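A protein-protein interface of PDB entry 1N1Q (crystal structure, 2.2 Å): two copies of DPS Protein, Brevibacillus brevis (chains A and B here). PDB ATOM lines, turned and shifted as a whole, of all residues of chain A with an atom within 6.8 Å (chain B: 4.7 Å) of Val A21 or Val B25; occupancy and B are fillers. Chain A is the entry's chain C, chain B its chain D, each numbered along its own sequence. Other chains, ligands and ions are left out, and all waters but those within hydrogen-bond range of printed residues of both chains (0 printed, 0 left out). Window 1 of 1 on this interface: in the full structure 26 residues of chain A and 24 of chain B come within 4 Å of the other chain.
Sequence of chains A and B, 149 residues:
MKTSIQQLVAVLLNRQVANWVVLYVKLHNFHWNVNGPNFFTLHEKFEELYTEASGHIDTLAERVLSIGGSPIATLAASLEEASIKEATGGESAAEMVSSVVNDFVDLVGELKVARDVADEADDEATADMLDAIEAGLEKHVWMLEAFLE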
ATOM      1  N   GLN A  16      13.289 -14.700   8.361  1.00  0.00           N
ATOM      2  CA  GLN A  16      13.486 -15.784   9.314  1.00  0.00           C
ATOM      3  C   GLN A  16      12.464 -16.894   9.088  1.00  0.00           C
ATOM      4  O   GLN A  16      12.734 -18.064   9.364  1.00  0.00           O
ATOM      5  CB  GLN A  16      13.413 -15.248  10.743  1.00  0.00           C
ATOM      6  CG  GLN A  16      14.503 -14.221  11.046  1.00  0.00           C
ATOM      7  CD  GLN A  16      15.872 -14.669  10.558  1.00  0.00           C
ATOM      8  OE1 GLN A  16      16.302 -15.794  10.829  1.00  0.00           O
ATOM      9  NE2 GLN A  16      16.566 -13.785   9.839  1.00  0.00           N
ATOM     10  N   VAL A  17      11.285 -16.529   8.592  1.00  0.00           N
ATOM     11  CA  VAL A  17      10.268 -17.526   8.289  1.00  0.00           C
ATOM     12  C   VAL A  17      10.875 -18.414   7.208  1.00  0.00           C
ATOM     13  O   VAL A  17      10.810 -19.634   7.284  1.00  0.00           O
ATOM     14  CB  VAL A  17       8.964 -16.888   7.735  1.00  0.00           C
ATOM     15  CG1 VAL A  17       8.073 -17.972   7.123  1.00  0.00           C
ATOM     16  CG2 VAL A  17       8.203 -16.177   8.850  1.00  0.00           C
ATOM     17  N   ALA A  18      11.491 -17.787   6.213  1.00  0.00           N
ATOM     18  CA  ALA A  18      12.124 -18.516   5.124  1.00  0.00           C
ATOM     19  C   ALA A  18      13.264 -19.390   5.643  1.00  0.00           C
ATOM     20  O   ALA A  18      13.380 -20.559   5.271  1.00  0.00           O
ATOM     21  CB  ALA A  18      12.649 -17.538   4.066  1.00  0.00           C
ATOM     22  N   ASN A  19      14.093 -18.825   6.518  1.00  0.00           N
ATOM     23  CA  ASN A  19      15.217 -19.568   7.082  1.00  0.00           C
ATOM     24  C   ASN A  19      14.771 -20.815   7.832  1.00  0.00           C
ATOM     25  O   ASN A  19      15.348 -21.891   7.658  1.00  0.00           O
ATOM     26  CB  ASN A  19      16.031 -18.693   8.034  1.00  0.00           C
ATOM     27  CG  ASN A  19      16.974 -17.761   7.298  1.00  0.00           C
ATOM     28  OD1 ASN A  19      17.379 -18.049   6.175  1.00  0.00           O
ATOM     29  ND2 ASN A  19      17.346 -16.654   7.936  1.00  0.00           N
ATOM     30  N   TRP A  20      13.748 -20.674   8.667  1.00  0.00           N
ATOM     31  CA  TRP A  20      13.258 -21.808   9.438  1.00  0.00           C
ATOM     32  C   TRP A  20      12.494 -22.834   8.612  1.00  0.00           C
ATOM     33  O   TRP A  20      12.428 -24.005   8.982  1.00  0.00           O
ATOM     34  CB  TRP A  20      12.428 -21.310  10.625  1.00  0.00           C
ATOM     35  CG  TRP A  20      13.315 -20.796  11.714  1.00  0.00           C
ATOM     36  CD1 TRP A  20      13.533 -19.491  12.055  1.00  0.00           C
ATOM     37  CD2 TRP A  20      14.184 -21.579  12.537  1.00  0.00           C
ATOM     38  NE1 TRP A  20      14.490 -19.412  13.041  1.00  0.00           N
ATOM     39  CE2 TRP A  20      14.910 -20.680  13.353  1.00  0.00           C
ATOM     40  CE3 TRP A  20      14.424 -22.954  12.662  1.00  0.00           C
ATOM     41  CZ2 TRP A  20      15.862 -21.114  14.285  1.00  0.00           C
ATOM     42  CZ3 TRP A  20      15.371 -23.388  13.588  1.00  0.00           C
ATOM     43  CH2 TRP A  20      16.078 -22.470  14.387  1.00  0.00           C
ATOM     44  N   VAL A  21      11.916 -22.399   7.498  1.00  0.00           N
ATOM     45  CA  VAL A  21      11.209 -23.326   6.620  1.00  0.00           C
ATOM     46  C   VAL A  21      12.296 -24.193   5.986  1.00  0.00           C
ATOM     47  O   VAL A  21      12.141 -25.405   5.831  1.00  0.00           O
ATOM     48  CB  VAL A  21      10.412 -22.587   5.505  1.00  0.00           C
ATOM     49  CG1 VAL A  21       9.744 -23.599   4.579  1.00  0.00           C
ATOM     50  CG2 VAL A  21       9.362 -21.699   6.125  1.00  0.00           C
ATOM     51  N   VAL A  22      13.407 -23.564   5.625  1.00  0.00           N
ATOM     52  CA  VAL A  22      14.526 -24.297   5.049  1.00  0.00           C
ATOM     53  C   VAL A  22      15.104 -25.240   6.109  1.00  0.00           C
ATOM     54  O   VAL A  22      15.325 -26.422   5.850  1.00  0.00           O
ATOM     55  CB  VAL A  22      15.643 -23.336   4.562  1.00  0.00           C
ATOM     56  CG1 VAL A  22      16.940 -24.114   4.318  1.00  0.00           C
ATOM     57  CG2 VAL A  22      15.203 -22.629   3.281  1.00  0.00           C
ATOM     58  N   LEU A  23      15.318 -24.714   7.311  1.00  0.00           N
ATOM     59  CA  LEU A  23      15.883 -25.511   8.400  1.00  0.00           C
ATOM     60  C   LEU A  23      15.016 -26.686   8.833  1.00  0.00           C
ATOM     61  O   LEU A  23      15.537 -27.724   9.241  1.00  0.00           O
ATOM     62  CB  LEU A  23      16.190 -24.626   9.609  1.00  0.00           C
ATOM     63  CG  LEU A  23      17.519 -23.864   9.490  1.00  0.00           C
ATOM     64  CD1 LEU A  23      17.618 -22.796  10.570  1.00  0.00           C
ATOM     65  CD2 LEU A  23      18.680 -24.855   9.596  1.00  0.00           C
ATOM     66  N   TYR A  24      13.697 -26.536   8.746  1.00  0.00           N
ATOM     67  CA  TYR A  24      12.810 -27.626   9.123  1.00  0.00           C
ATOM     68  C   TYR A  24      13.165 -28.852   8.282  1.00  0.00           C
ATOM     69  O   TYR A  24      13.224 -29.968   8.786  1.00  0.00           O
ATOM     70  CB  TYR A  24      11.349 -27.235   8.882  1.00  0.00           C
ATOM     71  CG  TYR A  24      10.364 -28.346   9.176  1.00  0.00           C
ATOM     72  CD1 TYR A  24      10.045 -28.699  10.491  1.00  0.00           C
ATOM     73  CD2 TYR A  24       9.750 -29.050   8.137  1.00  0.00           C
ATOM     74  CE1 TYR A  24       9.140 -29.718  10.761  1.00  0.00           C
ATOM     75  CE2 TYR A  24       8.845 -30.077   8.401  1.00  0.00           C
ATOM     76  CZ  TYR A  24       8.543 -30.403   9.713  1.00  0.00           C
ATOM     77  OH  TYR A  24       7.642 -31.412   9.971  1.00  0.00           O
ATOM     78  N   VAL A  25      13.403 -28.638   6.994  1.00  0.00           N
ATOM     79  CA  VAL A  25      13.758 -29.743   6.112  1.00  0.00           C
ATOM     80  C   VAL A  25      15.232 -30.136   6.226  1.00  0.00           C
ATOM     81  O   VAL A  25      15.568 -31.310   6.096  1.00  0.00           O
ATOM     82  CB  VAL A  25      13.407 -29.410   4.644  1.00  0.00           C
ATOM     83  CG1 VAL A  25      14.088 -30.399   3.677  1.00  0.00           C
ATOM     84  CG2 VAL A  25      11.909 -29.496   4.462  1.00  0.00           C
ATOM     85  N   LYS A  26      16.099 -29.163   6.494  1.00  0.00           N
ATOM     86  CA  LYS A  26      17.525 -29.444   6.630  1.00  0.00           C
ATOM     87  C   LYS A  26      17.777 -30.322   7.862  1.00  0.00           C
ATOM     88  O   LYS A  26      18.565 -31.264   7.826  1.00  0.00           O
ATOM     89  CB  LYS A  26      18.309 -28.137   6.745  1.00  0.00           C
ATOM     90  CG  LYS A  26      19.826 -28.289   6.577  1.00  0.00           C
ATOM     91  CD  LYS A  26      20.504 -26.923   6.563  1.00  0.00           C
ATOM     92  CE  LYS A  26      21.995 -27.023   6.234  1.00  0.00           C
ATOM     93  NZ  LYS A  26      22.625 -25.667   6.181  1.00  0.00           N
ATOM     94  N   ALA A  53      11.985 -25.901  15.158  1.00  0.00           N
ATOM     95  CA  ALA A  53      11.886 -25.180  13.888  1.00  0.00           C
ATOM     96  C   ALA A  53      10.423 -25.000  13.523  1.00  0.00           C
ATOM     97  O   ALA A  53       9.995 -23.918  13.124  1.00  0.00           O
ATOM     98  CB  ALA A  53      12.602 -25.953  12.781  1.00  0.00           C
ATOM     99  N   ILE A  57       8.541 -21.374  12.859  1.00  0.00           N
ATOM    100  CA  ILE A  57       7.832 -21.081  11.618  1.00  0.00           C
ATOM    101  C   ILE A  57       6.470 -20.460  11.903  1.00  0.00           C
ATOM    102  O   ILE A  57       6.135 -19.405  11.355  1.00  0.00           O
ATOM    103  CB  ILE A  57       7.576 -22.353  10.777  1.00  0.00           C
ATOM    104  CG1 ILE A  57       8.896 -22.969  10.301  1.00  0.00           C
ATOM    105  CG2 ILE A  57       6.722 -21.992   9.554  1.00  0.00           C
ATOM    106  CD1 ILE A  57       9.580 -22.129   9.279  1.00  0.00           C
ATOM    107  N   ILE A  72       5.713 -15.462   4.444  1.00  0.00           N
ATOM    108  CA  ILE A  72       6.209 -16.250   3.334  1.00  0.00           C
ATOM    109  C   ILE A  72       5.638 -17.630   3.586  1.00  0.00           C
ATOM    110  O   ILE A  72       5.777 -18.193   4.673  1.00  0.00           O
ATOM    111  CB  ILE A  72       7.738 -16.183   3.282  1.00  0.00           C
ATOM    112  CG1 ILE A  72       8.091 -14.898   2.502  1.00  0.00           C
ATOM    113  CG2 ILE A  72       8.357 -17.476   2.690  1.00  0.00           C
ATOM    114  CD1 ILE A  72       9.540 -14.486   2.576  1.00  0.00           C
ATOM    115  N   ALA A  73       4.948 -18.147   2.577  1.00  0.00           N
ATOM    116  CA  ALA A  73       4.276 -19.422   2.723  1.00  0.00           C
ATOM    117  C   ALA A  73       4.290 -20.350   1.518  1.00  0.00           C
ATOM    118  O   ALA A  73       3.262 -20.932   1.156  1.00  0.00           O
ATOM    119  CB  ALA A  73       2.829 -19.173   3.170  1.00  0.00           C
ATOM    120  N   THR A  74       5.458 -20.484   0.906  1.00  0.00           N
ATOM    121  CA  THR A  74       5.666 -21.373  -0.229  1.00  0.00           C
ATOM    122  C   THR A  74       7.130 -21.758  -0.137  1.00  0.00           C
ATOM    123  O   THR A  74       7.930 -21.016   0.443  1.00  0.00           O
ATOM    124  CB  THR A  74       5.436 -20.690  -1.607  1.00  0.00           C
ATOM    125  OG1 THR A  74       6.395 -19.644  -1.792  1.00  0.00           O
ATOM    126  CG2 THR A  74       4.017 -20.138  -1.708  1.00  0.00           C
ATOM    127  N   LEU A  75       7.487 -22.910  -0.692  1.00  0.00           N
ATOM    128  CA  LEU A  75       8.876 -23.340  -0.657  1.00  0.00           C
ATOM    129  C   LEU A  75       9.699 -22.480  -1.606  1.00  0.00           C
ATOM    130  O   LEU A  75      10.861 -22.188  -1.340  1.00  0.00           O
ATOM    131  CB  LEU A  75       8.999 -24.810  -1.059  1.00  0.00           C
ATOM    132  CG  LEU A  75       8.168 -25.838  -0.288  1.00  0.00           C
ATOM    133  CD1 LEU A  75       8.682 -27.228  -0.616  1.00  0.00           C
ATOM    134  CD2 LEU A  75       8.264 -25.577   1.207  1.00  0.00           C
ATOM    135  N   SER A  78      10.526 -19.311   0.102  1.00  0.00           N
ATOM    136  CA  SER A  78      11.430 -19.578   1.218  1.00  0.00           C
ATOM    137  C   SER A  78      12.859 -19.721   0.700  1.00  0.00           C
ATOM    138  O   SER A  78      13.801 -19.138   1.244  1.00  0.00           O
ATOM    139  CB  SER A  78      11.002 -20.855   1.953  1.00  0.00           C
ATOM    140  OG  SER A  78       9.769 -20.658   2.627  1.00  0.00           O
ATOM    141  N   LEU A  79      13.014 -20.502  -0.361  1.00  0.00           N
ATOM    142  CA  LEU A  79      14.321 -20.724  -0.967  1.00  0.00           C
ATOM    143  C   LEU A  79      14.894 -19.404  -1.471  1.00  0.00           C
ATOM    144  O   LEU A  79      16.092 -19.132  -1.369  1.00  0.00           O
ATOM    145  CB  LEU A  79      14.204 -21.689  -2.147  1.00  0.00           C
ATOM    146  CG  LEU A  79      14.186 -23.175  -1.801  1.00  0.00           C
ATOM    147  CD1 LEU A  79      13.880 -23.998  -3.041  1.00  0.00           C
ATOM    148  CD2 LEU A  79      15.539 -23.560  -1.212  1.00  0.00           C
ATOM    149  N   GLU A  86      20.599 -25.275   1.893  1.00  0.00           N
ATOM    150  CA  GLU A  86      20.091 -26.618   2.106  1.00  0.00           C
ATOM    151  C   GLU A  86      21.246 -27.594   2.247  1.00  0.00           C
ATOM    152  O   GLU A  86      22.356 -27.311   1.812  1.00  0.00           O
ATOM    153  CB  GLU A  86      19.184 -27.014   0.940  1.00  0.00           C
ATOM    154  CG  GLU A  86      18.076 -26.002   0.696  1.00  0.00           C
ATOM    155  CD  GLU A  86      16.820 -26.642   0.161  1.00  0.00           C
ATOM    156  OE1 GLU A  86      16.677 -26.750  -1.082  1.00  0.00           O
ATOM    157  OE2 GLU A  86      15.976 -27.049   0.992  1.00  0.00           O
ATOM    158  N   VAL B  21       6.075 -32.515   1.880  1.00  0.00           N
ATOM    159  CA  VAL B  21       6.952 -31.412   2.273  1.00  0.00           C
ATOM    160  C   VAL B  21       6.290 -30.144   1.733  1.00  0.00           C
ATOM    161  O   VAL B  21       6.256 -29.113   2.401  1.00  0.00           O
ATOM    162  CB  VAL B  21       8.377 -31.564   1.664  1.00  0.00           C
ATOM    163  CG1 VAL B  21       9.249 -30.350   2.023  1.00  0.00           C
ATOM    164  CG2 VAL B  21       9.023 -32.820   2.187  1.00  0.00           C
ATOM    165  N   VAL B  22       5.752 -30.235   0.521  1.00  0.00           N
ATOM    166  CA  VAL B  22       5.055 -29.106  -0.083  1.00  0.00           C
ATOM    167  C   VAL B  22       3.788 -28.806   0.730  1.00  0.00           C
ATOM    168  O   VAL B  22       3.523 -27.655   1.081  1.00  0.00           O
ATOM    169  CB  VAL B  22       4.647 -29.410  -1.548  1.00  0.00           C
ATOM    170  CG1 VAL B  22       3.602 -28.393  -2.031  1.00  0.00           C
ATOM    171  CG2 VAL B  22       5.874 -29.358  -2.455  1.00  0.00           C
ATOM    172  N   LEU B  23       3.018 -29.847   1.040  1.00  0.00           N
ATOM    173  CA  LEU B  23       1.783 -29.685   1.802  1.00  0.00           C
ATOM    174  C   LEU B  23       1.988 -29.137   3.210  1.00  0.00           C
ATOM    175  O   LEU B  23       1.129 -28.414   3.725  1.00  0.00           O
ATOM    176  CB  LEU B  23       1.017 -31.009   1.868  1.00  0.00           C
ATOM    177  CG  LEU B  23       0.192 -31.314   0.603  1.00  0.00           C
ATOM    178  CD1 LEU B  23      -0.284 -32.759   0.613  1.00  0.00           C
ATOM    179  CD2 LEU B  23      -0.996 -30.353   0.532  1.00  0.00           C
ATOM    180  N   TYR B  24       3.108 -29.478   3.842  1.00  0.00           N
ATOM    181  CA  TYR B  24       3.369 -28.972   5.186  1.00  0.00           C
ATOM    182  C   TYR B  24       3.317 -27.443   5.146  1.00  0.00           C
ATOM    183  O   TYR B  24       2.740 -26.807   6.021  1.00  0.00           O
ATOM    184  CB  TYR B  24       4.738 -29.438   5.677  1.00  0.00           C
ATOM    185  CG  TYR B  24       5.117 -28.892   7.041  1.00  0.00           C
ATOM    186  CD1 TYR B  24       4.537 -29.401   8.207  1.00  0.00           C
ATOM    187  CD2 TYR B  24       6.057 -27.867   7.168  1.00  0.00           C
ATOM    188  CE1 TYR B  24       4.888 -28.900   9.467  1.00  0.00           C
ATOM    189  CE2 TYR B  24       6.410 -27.363   8.414  1.00  0.00           C
ATOM    190  CZ  TYR B  24       5.826 -27.881   9.557  1.00  0.00           C
ATOM    191  OH  TYR B  24       6.175 -27.384  10.792  1.00  0.00           O
ATOM    192  N   VAL B  25       3.914 -26.858   4.115  1.00  0.00           N
ATOM    193  CA  VAL B  25       3.920 -25.406   3.983  1.00  0.00           C
ATOM    194  C   VAL B  25       2.612 -24.861   3.414  1.00  0.00           C
ATOM    195  O   VAL B  25       2.168 -23.779   3.787  1.00  0.00           O
ATOM    196  CB  VAL B  25       5.120 -24.935   3.123  1.00  0.00           C
ATOM    197  CG1 VAL B  25       4.939 -23.480   2.681  1.00  0.00           C
ATOM    198  CG2 VAL B  25       6.395 -25.056   3.945  1.00  0.00           C
ATOM    199  N   LYS B  26       1.980 -25.619   2.529  1.00  0.00           N
ATOM    200  CA  LYS B  26       0.719 -25.190   1.935  1.00  0.00           C
ATOM    201  C   LYS B  26      -0.373 -25.106   3.006  1.00  0.00           C
ATOM    202  O   LYS B  26      -1.172 -24.164   3.032  1.00  0.00           O
ATOM    203  CB  LYS B  26       0.300 -26.169   0.830  1.00  0.00           C
ATOM    204  CG  LYS B  26      -0.820 -25.640  -0.085  1.00  0.00           C
ATOM    205  CD  LYS B  26      -1.080 -26.624  -1.228  1.00  0.00           C
ATOM    206  CE  LYS B  26      -2.080 -26.079  -2.248  1.00  0.00           C
ATOM    207  NZ  LYS B  26      -2.241 -27.040  -3.397  1.00  0.00           N
ATOM    208  N   LEU B  27      -0.398 -26.098   3.887  1.00  0.00           N
ATOM    209  CA  LEU B  27      -1.377 -26.139   4.962  1.00  0.00           C
ATOM    210  C   LEU B  27      -1.112 -25.013   5.964  1.00  0.00           C
ATOM    211  O   LEU B  27      -2.036 -24.487   6.583  1.00  0.00           O
ATOM    212  CB  LEU B  27      -1.340 -27.508   5.641  1.00  0.00           C
ATOM    213  CG  LEU B  27      -1.854 -28.615   4.710  1.00  0.00           C
ATOM    214  CD1 LEU B  27      -1.489 -29.986   5.255  1.00  0.00           C
ATOM    215  CD2 LEU B  27      -3.373 -28.479   4.557  1.00  0.00           C
ATOM    216  N   HIS B  28       0.157 -24.653   6.131  1.00  0.00           N
ATOM    217  CA  HIS B  28       0.522 -23.543   7.016  1.00  0.00           C
ATOM    218  C   HIS B  28      -0.018 -22.277   6.367  1.00  0.00           C
ATOM    219  O   HIS B  28      -0.562 -21.399   7.039  1.00  0.00           O
ATOM    220  CB  HIS B  28       2.045 -23.440   7.153  1.00  0.00           C
ATOM    221  CG  HIS B  28       2.598 -24.172   8.337  1.00  0.00           C
ATOM    222  ND1 HIS B  28       2.608 -23.634   9.606  1.00  0.00           N
ATOM    223  CD2 HIS B  28       3.152 -25.402   8.448  1.00  0.00           C
ATOM    224  CE1 HIS B  28       3.148 -24.500  10.446  1.00  0.00           C
ATOM    225  NE2 HIS B  28       3.486 -25.581   9.769  1.00  0.00           N
ATOM    226  N   ASN B  29       0.120 -22.207   5.044  1.00  0.00           N
ATOM    227  CA  ASN B  29      -0.353 -21.059   4.280  1.00  0.00           C
ATOM    228  C   ASN B  29      -1.839 -20.835   4.553  1.00  0.00           C
ATOM    229  O   ASN B  29      -2.268 -19.725   4.861  1.00  0.00           O
ATOM    230  CB  ASN B  29      -0.127 -21.297   2.782  1.00  0.00           C
ATOM    231  CG  ASN B  29      -0.476 -20.088   1.934  1.00  0.00           C
ATOM    232  OD1 ASN B  29      -1.585 -19.564   2.006  1.00  0.00           O
ATOM    233  ND2 ASN B  29       0.477 -19.642   1.119  1.00  0.00           N
ATOM    234  N   LEU B  75      14.213 -28.462  -0.209  1.00  0.00           N
ATOM    235  CA  LEU B  75      13.012 -27.857  -0.752  1.00  0.00           C
ATOM    236  C   LEU B  75      13.082 -27.885  -2.267  1.00  0.00           C
ATOM    237  O   LEU B  75      12.066 -28.061  -2.939  1.00  0.00           O
ATOM    238  CB  LEU B  75      12.867 -26.410  -0.264  1.00  0.00           C
ATOM    239  CG  LEU B  75      12.857 -26.166   1.248  1.00  0.00           C
ATOM    240  CD1 LEU B  75      12.360 -24.752   1.509  1.00  0.00           C
ATOM    241  CD2 LEU B  75      11.958 -27.177   1.941  1.00  0.00           C
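Printed residues of chain B that touch a printed residue of chain A: Val B21, Val B22, Tyr B24, Val B25, Asn B29 and Leu B75. Hydrophobic or aromatic side chains of chain B within 4 Å of the printed part of chain A: Val B21, Val B22, Tyr B24, Val B25 and Leu B75. Hydrophobic or aromatic side chains of chain A within 4 Å of the printed part of chain B: Val A21, Val A22, Tyr A24, Val A25, Ala A73, Leu A75 and Leu A79. Among the printed residues, 12 pairs touch across the chains. Among the printed residues, no Asp or Glu carboxylate lies within 4 Å of a Lys or Arg side-chain nitrogen of the other chain.
Val A21 touches Val B25. CD1 of Leu B75 touches CG2 of Val A22, at 3.97 Å. Tyr A24 touches Tyr B24. Val A25 touches Val B21. Val A25 touches Leu B75. Ala A73 touches Val B25 (C to CG1, 3.4 Å). Thr A74 touches Val B25. Leu A75 touches Val B22 (CD1 to CG2, 3.98 Å). Leu A75 touches Val B25. Leu B75 touches Leu A79 (CB to CD1, 3.8 Å).
Val A21 touches Val B25, and with the chains exchanged Val A25 touches Val B21. Val A22 touches Leu B75, and with the chains exchanged Leu A75 touches Val B22. Tyr B24 touches its own counterpart, Tyr A24. Val A25 touches Leu B75, and with the chains exchanged Leu A75 touches Val B25. 7 positions are printed for both chains. Of the 12 pairs that touch across the chains among the printed residues, 7 have their exchanged pair printed and touching as well.
OG of Ser A78 lies within hydrogen-bond range of O of Thr A74 (2.9 Å). A ring nitrogen (NE2) of His B28 lies close to the side-chain hydroxyl (OH) of Tyr B24 (3.4 Å).
Of chain B, only Val B25 comes within 4 Å of Val A21. Of the printed residues of chain B, Tyr A24 touches Tyr B24. Ser A78 touches none of the printed residues of chain B. Printed residues of chain B within 4 Å of Glu A86: Leu B75 (2.6 Å). Lys B26 touches none of the printed residues of chain A. Of the printed residues of chain A, Asn B29 touches Ala A73 (3.1 Å). Of the printed residues of chain A, Leu B75 touches Val A22 (3.97 Å), Val A25 (3.4 Å), Leu A79 (3.8 Å) and Glu A86 (2.6 Å). The nearest residue of chain B that does not touch Val A21 is Leu B75 (4.2 Å).
The side-chain amide nitrogen of Asn B29 is in hydrogen-bond range of the backbone carbonyl oxygen of Ala A73. The side-chain carboxylate (OE2) of Glu A86 is in hydrogen-bond range of the backbone NH (N) of Leu B75 (2.6 Å).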
